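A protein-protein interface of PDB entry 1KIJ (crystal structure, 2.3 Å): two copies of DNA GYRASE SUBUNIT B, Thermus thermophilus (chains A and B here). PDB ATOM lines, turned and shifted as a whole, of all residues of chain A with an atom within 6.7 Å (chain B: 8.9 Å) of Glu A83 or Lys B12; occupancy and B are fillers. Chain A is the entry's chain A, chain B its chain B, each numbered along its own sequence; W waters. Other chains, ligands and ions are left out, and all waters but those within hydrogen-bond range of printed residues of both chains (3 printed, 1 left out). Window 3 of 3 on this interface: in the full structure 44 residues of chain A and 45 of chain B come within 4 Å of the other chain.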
ATOM      1  N   MET A  80      28.946  11.805  10.399  1.00  0.00           N
ATOM      2  CA  MET A  80      29.200  11.926  11.825  1.00  0.00           C
ATOM      3  C   MET A  80      29.500  10.484  12.208  1.00  0.00           C
ATOM      4  O   MET A  80      28.596   9.673  12.333  1.00  0.00           O
ATOM      5  CB  MET A  80      27.961  12.431  12.563  1.00  0.00           C
ATOM      6  CG  MET A  80      27.801  13.939  12.530  1.00  0.00           C
ATOM      7  SD  MET A  80      26.419  14.514  13.543  1.00  0.00           S
ATOM      8  CE  MET A  80      26.942  13.926  15.188  1.00  0.00           C
ATOM      9  N   PRO A  81      30.789  10.152  12.378  1.00  0.00           N
ATOM     10  CA  PRO A  81      31.221   8.798  12.736  1.00  0.00           C
ATOM     11  C   PRO A  81      30.410   8.133  13.847  1.00  0.00           C
ATOM     12  O   PRO A  81      30.045   6.963  13.746  1.00  0.00           O
ATOM     13  CB  PRO A  81      32.691   8.994  13.109  1.00  0.00           C
ATOM     14  CG  PRO A  81      32.726  10.406  13.617  1.00  0.00           C
ATOM     15  CD  PRO A  81      31.883  11.116  12.590  1.00  0.00           C
ATOM     16  N   GLU A  82      30.124   8.896  14.897  1.00  0.00           N
ATOM     17  CA  GLU A  82      29.370   8.402  16.041  1.00  0.00           C
ATOM     18  C   GLU A  82      27.973   7.877  15.689  1.00  0.00           C
ATOM     19  O   GLU A  82      27.447   7.011  16.384  1.00  0.00           O
ATOM     20  CB  GLU A  82      29.252   9.513  17.090  1.00  0.00           C
ATOM     21  CG  GLU A  82      29.593   9.073  18.503  1.00  0.00           C
ATOM     22  CD  GLU A  82      31.072   8.770  18.680  1.00  0.00           C
ATOM     23  OE1 GLU A  82      31.442   8.189  19.722  1.00  0.00           O
ATOM     24  OE2 GLU A  82      31.869   9.119  17.783  1.00  0.00           O
ATOM     25  N   GLU A  83      27.376   8.397  14.617  1.00  0.00           N
ATOM     26  CA  GLU A  83      26.035   7.972  14.211  1.00  0.00           C
ATOM     27  C   GLU A  83      25.967   7.278  12.848  1.00  0.00           C
ATOM     28  O   GLU A  83      24.963   6.667  12.518  1.00  0.00           O
ATOM     29  CB  GLU A  83      25.079   9.173  14.207  1.00  0.00           C
ATOM     30  CG  GLU A  83      24.970   9.927  15.536  1.00  0.00           C
ATOM     31  CD  GLU A  83      24.520   9.046  16.696  1.00  0.00           C
ATOM     32  OE1 GLU A  83      23.522   8.308  16.542  1.00  0.00           O
ATOM     33  OE2 GLU A  83      25.158   9.098  17.771  1.00  0.00           O
ATOM     34  N   GLY A  84      27.030   7.377  12.057  1.00  0.00           N
ATOM     35  CA  GLY A  84      27.038   6.746  10.746  1.00  0.00           C
ATOM     36  C   GLY A  84      26.056   7.357   9.760  1.00  0.00           C
ATOM     37  O   GLY A  84      25.478   6.658   8.924  1.00  0.00           O
ATOM     38  N   LYS A  85      25.864   8.668   9.854  1.00  0.00           N
ATOM     39  CA  LYS A  85      24.945   9.376   8.968  1.00  0.00           C
ATOM     40  C   LYS A  85      25.484  10.764   8.679  1.00  0.00           C
ATOM     41  O   LYS A  85      26.201  11.341   9.488  1.00  0.00           O
ATOM     42  CB  LYS A  85      23.569   9.515   9.619  1.00  0.00           C
ATOM     43  CG  LYS A  85      22.880   8.208   9.950  1.00  0.00           C
ATOM     44  CD  LYS A  85      21.772   8.441  10.974  1.00  0.00           C
ATOM     45  CE  LYS A  85      21.042   7.154  11.332  1.00  0.00           C
ATOM     46  NZ  LYS A  85      20.057   7.374  12.432  1.00  0.00           N
ATOM     47  N   VAL A  90      21.352  13.903  10.687  1.00  0.00           N
ATOM     48  CA  VAL A  90      21.322  13.955  12.152  1.00  0.00           C
ATOM     49  C   VAL A  90      20.579  15.192  12.666  1.00  0.00           C
ATOM     50  O   VAL A  90      19.674  15.089  13.470  1.00  0.00           O
ATOM     51  CB  VAL A  90      22.765  13.971  12.731  1.00  0.00           C
ATOM     52  CG1 VAL A  90      22.742  14.344  14.200  1.00  0.00           C
ATOM     53  CG2 VAL A  90      23.417  12.601  12.543  1.00  0.00           C
ATOM     54  N   THR A  94      17.186  14.004  14.771  1.00  0.00           N
ATOM     55  CA  THR A  94      17.377  13.705  16.182  1.00  0.00           C
ATOM     56  C   THR A  94      16.786  14.857  16.977  1.00  0.00           C
ATOM     57  O   THR A  94      16.940  16.027  16.624  1.00  0.00           O
ATOM     58  CB  THR A  94      18.871  13.526  16.588  1.00  0.00           C
ATOM     59  OG1 THR A  94      19.408  14.782  17.013  1.00  0.00           O
ATOM     60  CG2 THR A  94      19.699  12.980  15.431  1.00  0.00           C
ATOM     61  N   HIS A  96      17.606  16.135  19.880  1.00  0.00           N
ATOM     62  CA  HIS A  96      18.571  17.083  20.419  1.00  0.00           C
ATOM     63  C   HIS A  96      20.030  16.803  20.087  1.00  0.00           C
ATOM     64  O   HIS A  96      20.624  15.874  20.597  1.00  0.00           O
ATOM     65  CB  HIS A  96      18.409  17.160  21.943  1.00  0.00           C
ATOM     66  CG  HIS A  96      19.207  18.251  22.596  1.00  0.00           C
ATOM     67  ND1 HIS A  96      19.161  18.492  23.952  1.00  0.00           N
ATOM     68  CD2 HIS A  96      20.049  19.179  22.082  1.00  0.00           C
ATOM     69  CE1 HIS A  96      19.935  19.521  24.246  1.00  0.00           C
ATOM     70  NE2 HIS A  96      20.485  19.958  23.129  1.00  0.00           N
ATOM     71  N   ILE B   8      29.994  18.225  16.930  1.00  0.00           N
ATOM     72  CA  ILE B   8      28.591  17.874  17.088  1.00  0.00           C
ATOM     73  C   ILE B   8      28.325  16.465  17.607  1.00  0.00           C
ATOM     74  O   ILE B   8      28.990  15.507  17.229  1.00  0.00           O
ATOM     75  CB  ILE B   8      27.845  18.061  15.740  1.00  0.00           C
ATOM     76  CG1 ILE B   8      26.348  17.803  15.913  1.00  0.00           C
ATOM     77  CG2 ILE B   8      28.431  17.130  14.692  1.00  0.00           C
ATOM     78  CD1 ILE B   8      25.532  18.128  14.688  1.00  0.00           C
ATOM     79  N   ARG B   9      27.328  16.363  18.480  1.00  0.00           N
ATOM     80  CA  ARG B   9      26.924  15.094  19.066  1.00  0.00           C
ATOM     81  C   ARG B   9      25.430  15.069  19.398  1.00  0.00           C
ATOM     82  O   ARG B   9      24.795  16.099  19.571  1.00  0.00           O
ATOM     83  CB  ARG B   9      27.733  14.810  20.336  1.00  0.00           C
ATOM     84  CG  ARG B   9      27.654  15.895  21.405  1.00  0.00           C
ATOM     85  CD  ARG B   9      28.180  15.371  22.740  1.00  0.00           C
ATOM     86  NE  ARG B   9      28.261  16.408  23.768  1.00  0.00           N
ATOM     87  CZ  ARG B   9      28.045  16.192  25.063  1.00  0.00           C
ATOM     88  NH1 ARG B   9      27.725  14.974  25.493  1.00  0.00           N
ATOM     89  NH2 ARG B   9      28.155  17.189  25.933  1.00  0.00           N
ATOM     90  N   VAL B  10      24.880  13.864  19.472  1.00  0.00           N
ATOM     91  CA  VAL B  10      23.479  13.668  19.797  1.00  0.00           C
ATOM     92  C   VAL B  10      23.350  13.461  21.304  1.00  0.00           C
ATOM     93  O   VAL B  10      24.006  12.616  21.876  1.00  0.00           O
ATOM     94  CB  VAL B  10      22.915  12.427  19.083  1.00  0.00           C
ATOM     95  CG1 VAL B  10      21.485  12.146  19.564  1.00  0.00           C
ATOM     96  CG2 VAL B  10      22.940  12.640  17.579  1.00  0.00           C
ATOM     97  N   LEU B  11      22.509  14.264  21.936  1.00  0.00           N
ATOM     98  CA  LEU B  11      22.285  14.148  23.368  1.00  0.00           C
ATOM     99  C   LEU B  11      20.999  13.345  23.521  1.00  0.00           C
ATOM    100  O   LEU B  11      19.938  13.781  23.102  1.00  0.00           O
ATOM    101  CB  LEU B  11      22.140  15.539  23.979  1.00  0.00           C
ATOM    102  CG  LEU B  11      23.424  16.350  23.784  1.00  0.00           C
ATOM    103  CD1 LEU B  11      23.125  17.835  23.805  1.00  0.00           C
ATOM    104  CD2 LEU B  11      24.429  15.960  24.859  1.00  0.00           C
ATOM    105  N   LYS B  12      21.109  12.156  24.099  1.00  0.00           N
ATOM    106  CA  LYS B  12      19.949  11.292  24.273  1.00  0.00           C
ATOM    107  C   LYS B  12      19.370  11.394  25.678  1.00  0.00           C
ATOM    108  O   LYS B  12      20.101  11.520  26.653  1.00  0.00           O
ATOM    109  CB  LYS B  12      20.338   9.843  23.966  1.00  0.00           C
ATOM    110  CG  LYS B  12      20.732   9.608  22.503  1.00  0.00           C
ATOM    111  CD  LYS B  12      21.276   8.194  22.280  1.00  0.00           C
ATOM    112  CE  LYS B  12      21.330   7.820  20.794  1.00  0.00           C
ATOM    113  NZ  LYS B  12      22.188   8.714  19.968  1.00  0.00           N
ATOM    114  N   GLY B  13      18.043  11.348  25.763  1.00  0.00           N
ATOM    115  CA  GLY B  13      17.370  11.424  27.048  1.00  0.00           C
ATOM    116  C   GLY B  13      17.767  12.606  27.912  1.00  0.00           C
ATOM    117  O   GLY B  13      17.939  13.717  27.424  1.00  0.00           O
ATOM    118  N   LEU B  14      17.924  12.348  29.209  1.00  0.00           N
ATOM    119  CA  LEU B  14      18.282  13.370  30.190  1.00  0.00           C
ATOM    120  C   LEU B  14      19.640  14.035  29.981  1.00  0.00           C
ATOM    121  O   LEU B  14      19.938  15.053  30.600  1.00  0.00           O
ATOM    122  CB  LEU B  14      18.217  12.770  31.593  1.00  0.00           C
ATOM    123  CG  LEU B  14      16.868  12.154  31.969  1.00  0.00           C
ATOM    124  CD1 LEU B  14      16.939  11.628  33.389  1.00  0.00           C
ATOM    125  CD2 LEU B  14      15.761  13.197  31.828  1.00  0.00           C
ATOM    126  N   GLU B  15      20.465  13.445  29.125  1.00  0.00           N
ATOM    127  CA  GLU B  15      21.774  14.001  28.809  1.00  0.00           C
ATOM    128  C   GLU B  15      21.592  15.436  28.308  1.00  0.00           C
ATOM    129  O   GLU B  15      22.306  16.345  28.708  1.00  0.00           O
ATOM    130  CB  GLU B  15      22.427  13.180  27.704  1.00  0.00           C
ATOM    131  CG  GLU B  15      23.717  12.507  28.083  1.00  0.00           C
ATOM    132  CD  GLU B  15      24.522  12.123  26.857  1.00  0.00           C
ATOM    133  OE1 GLU B  15      23.959  11.437  25.972  1.00  0.00           O
ATOM    134  OE2 GLU B  15      25.714  12.512  26.781  1.00  0.00           O
ATOM    135  N   GLY B  16      20.620  15.619  27.420  1.00  0.00           N
ATOM    136  CA  GLY B  16      20.356  16.932  26.869  1.00  0.00           C
ATOM    137  C   GLY B  16      19.966  17.958  27.910  1.00  0.00           C
ATOM    138  O   GLY B  16      20.290  19.134  27.774  1.00  0.00           O
ATOM    139  N   VAL B  17      19.262  17.523  28.948  1.00  0.00           N
ATOM    140  CA  VAL B  17      18.842  18.440  29.992  1.00  0.00           C
ATOM    141  C   VAL B  17      20.053  18.997  30.733  1.00  0.00           C
ATOM    142  O   VAL B  17      20.096  20.176  31.058  1.00  0.00           O
ATOM    143  CB  VAL B  17      17.909  17.750  30.990  1.00  0.00           C
ATOM    144  CG1 VAL B  17      17.471  18.729  32.050  1.00  0.00           C
ATOM    145  CG2 VAL B  17      16.690  17.189  30.257  1.00  0.00           C
ATOM    146  N   ARG B  18      21.041  18.152  30.998  1.00  0.00           N
ATOM    147  CA  ARG B  18      22.223  18.631  31.697  1.00  0.00           C
ATOM    148  C   ARG B  18      23.143  19.419  30.770  1.00  0.00           C
ATOM    149  O   ARG B  18      23.915  20.240  31.223  1.00  0.00           O
ATOM    150  CB  ARG B  18      22.977  17.468  32.351  1.00  0.00           C
ATOM    151  CG  ARG B  18      22.254  16.908  33.582  1.00  0.00           C
ATOM    152  CD  ARG B  18      23.109  15.901  34.338  1.00  0.00           C
ATOM    153  NE  ARG B  18      24.323  16.504  34.888  1.00  0.00           N
ATOM    154  CZ  ARG B  18      24.387  17.228  36.005  1.00  0.00           C
ATOM    155  NH1 ARG B  18      23.305  17.456  36.732  1.00  0.00           N
ATOM    156  NH2 ARG B  18      25.551  17.734  36.395  1.00  0.00           N
ATOM    157  N   HIS B  19      23.038  19.177  29.467  1.00  0.00           N
ATOM    158  CA  HIS B  19      23.859  19.896  28.507  1.00  0.00           C
ATOM    159  C   HIS B  19      23.386  21.345  28.368  1.00  0.00           C
ATOM    160  O   HIS B  19      24.181  22.262  28.378  1.00  0.00           O
ATOM    161  CB  HIS B  19      23.825  19.210  27.137  1.00  0.00           C
ATOM    162  CG  HIS B  19      24.733  19.849  26.132  1.00  0.00           C
ATOM    163  ND1 HIS B  19      24.283  20.734  25.177  1.00  0.00           N
ATOM    164  CD2 HIS B  19      26.078  19.786  25.984  1.00  0.00           C
ATOM    165  CE1 HIS B  19      25.311  21.191  24.485  1.00  0.00           C
ATOM    166  NE2 HIS B  19      26.412  20.632  24.957  1.00  0.00           N
ATOM    167  N   TYR B  24      15.354  24.083  29.299  1.00  0.00           N
ATOM    168  CA  TYR B  24      14.237  23.456  30.012  1.00  0.00           C
ATOM    169  C   TYR B  24      13.651  24.309  31.117  1.00  0.00           C
ATOM    170  O   TYR B  24      12.488  24.180  31.437  1.00  0.00           O
ATOM    171  CB  TYR B  24      14.665  22.121  30.621  1.00  0.00           C
ATOM    172  CG  TYR B  24      14.933  21.047  29.597  1.00  0.00           C
ATOM    173  CD1 TYR B  24      16.175  20.937  28.990  1.00  0.00           C
ATOM    174  CD2 TYR B  24      13.930  20.160  29.219  1.00  0.00           C
ATOM    175  CE1 TYR B  24      16.420  19.971  28.030  1.00  0.00           C
ATOM    176  CE2 TYR B  24      14.162  19.191  28.265  1.00  0.00           C
ATOM    177  CZ  TYR B  24      15.411  19.105  27.678  1.00  0.00           C
ATOM    178  OH  TYR B  24      15.654  18.146  26.744  1.00  0.00           O
ATOM    179  N   ASN B  93      13.362   8.802  35.255  1.00  0.00           N
ATOM    180  CA  ASN B  93      14.570   8.593  34.456  1.00  0.00           C
ATOM    181  C   ASN B  93      14.447   8.777  32.954  1.00  0.00           C
ATOM    182  O   ASN B  93      15.454   8.845  32.261  1.00  0.00           O
ATOM    183  CB  ASN B  93      15.140   7.202  34.745  1.00  0.00           C
ATOM    184  CG  ASN B  93      15.808   7.129  36.101  1.00  0.00           C
ATOM    185  OD1 ASN B  93      16.920   7.595  36.287  1.00  0.00           O
ATOM    186  ND2 ASN B  93      15.114   6.549  37.059  1.00  0.00           N
ATOM    187  N   THR B  94      13.226   8.835  32.442  1.00  0.00           N
ATOM    188  CA  THR B  94      13.053   9.027  31.012  1.00  0.00           C
ATOM    189  C   THR B  94      12.607  10.456  30.769  1.00  0.00           C
ATOM    190  O   THR B  94      11.747  10.983  31.470  1.00  0.00           O
ATOM    191  CB  THR B  94      12.010   8.053  30.409  1.00  0.00           C
ATOM    192  OG1 THR B  94      10.690   8.462  30.780  1.00  0.00           O
ATOM    193  CG2 THR B  94      12.251   6.639  30.914  1.00  0.00           C
ATOM    194  N   LEU B  95      13.215  11.078  29.771  1.00  0.00           N
ATOM    195  CA  LEU B  95      12.910  12.458  29.407  1.00  0.00           C
ATOM    196  C   LEU B  95      11.413  12.659  29.158  1.00  0.00           C
ATOM    197  O   LEU B  95      10.818  13.593  29.661  1.00  0.00           O
ATOM    198  CB  LEU B  95      13.674  12.830  28.132  1.00  0.00           C
ATOM    199  CG  LEU B  95      14.120  14.273  27.862  1.00  0.00           C
ATOM    200  CD1 LEU B  95      13.972  14.553  26.369  1.00  0.00           C
ATOM    201  CD2 LEU B  95      13.312  15.264  28.670  1.00  0.00           C
ATOM    202  N   GLU B 146      20.343   9.607  37.080  1.00  0.00           N
ATOM    203  CA  GLU B 146      20.619   8.168  37.138  1.00  0.00           C
ATOM    204  C   GLU B 146      20.246   7.545  38.481  1.00  0.00           C
ATOM    205  O   GLU B 146      20.327   8.185  39.503  1.00  0.00           O
ATOM    206  CB  GLU B 146      22.111   7.913  36.881  1.00  0.00           C
ATOM    207  CG  GLU B 146      22.709   8.688  35.710  1.00  0.00           C
ATOM    208  CD  GLU B 146      22.916   7.839  34.470  1.00  0.00           C
ATOM    209  OE1 GLU B 146      23.370   8.398  33.448  1.00  0.00           O
ATOM    210  OE2 GLU B 146      22.635   6.615  34.513  1.00  0.00           O
HETATM  211  O   HOH W   1      26.697  11.692  18.807  1.00  0.00           O
HETATM  212  O   HOH W   2      22.394  22.102  23.090  1.00  0.00           O
HETATM  213  O   HOH W   3      18.246  13.390  20.677  1.00  0.00           O
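The side-chain carboxylate (OE1) of Glu A83 is in salt-bridge range of the side-chain amino group (NZ) of Lys B12, at 3.7 Å. O of His A96 sits at hydrogen-bond distance from N of Leu B11 (2.8 Å).
The backbone carbonyl oxygen of Lys A85 lies within hydrogen-bond range of the backbone NH of Met A80 (2.9 Å). OE1 of Glu B15 is in hydrogen-bond range of N of Lys B12, at 3.5 Å.
Among the printed residues, pairs that only touch across the chains: Met A80 with Ile B8 (3.3 Å), His A96 with Gly B16 (3.5 Å), His A96 with Val B10 (3.7 Å), Val A90 with Val B10 (3.8 Å), Thr A94 with Val B10 (3.9 Å) and Glu A83 with Val B10 (3.96 Å).
Of chain B, only Val B10 and Lys B12 come within 4 Å of Glu A83. Lys B12 touches one residue of chain A. Printed residues of chain A within 4 Å of Val B10: Glu A83 (3.96 Å), Val A90 (3.8 Å), Thr A94 (3.9 Å) and His A96 (3.7 Å). Printed residues of chain B within 4 Å of His A96: Val B10 (3.7 Å), Leu B11 (2.8 Å) and Gly B16 (3.5 Å). Printed residues of chain B within 4 Å of Met A80: Ile B8 (3.3 Å). Of the printed residues of chain B, Val A90 touches Val B10 (3.8 Å). His B19 touches none of the printed residues of chain A. Pro A81 touches none of the printed residues of chain B. The nearest residue of chain B that does not touch Glu A83 is Arg B9 (6.2 Å).
Of the 9 printed residues of chain A, 5 touch a printed residue of chain B. Hydrophobic or aromatic side chains of chain A within 4 Å of the printed part of chain B: Met A80, Val A90 and His A96. Among the printed residues, 8 pairs touch across the chains.
1 position is printed for both chains.
Water W2 bridges a ring nitrogen (NE2) of His A96 (2.9 Å) and a ring nitrogen (ND1) of His B19 (3.1 Å). Water W1 lies within hydrogen-bond range of the backbone NH of Val B10 (2.9 Å) and the side-chain carboxylate of Glu A83 (3.2 Å). Water W3 lies within hydrogen-bond range of N of His A96 (2.9 Å) and O of Leu B11 (3.0 Å).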
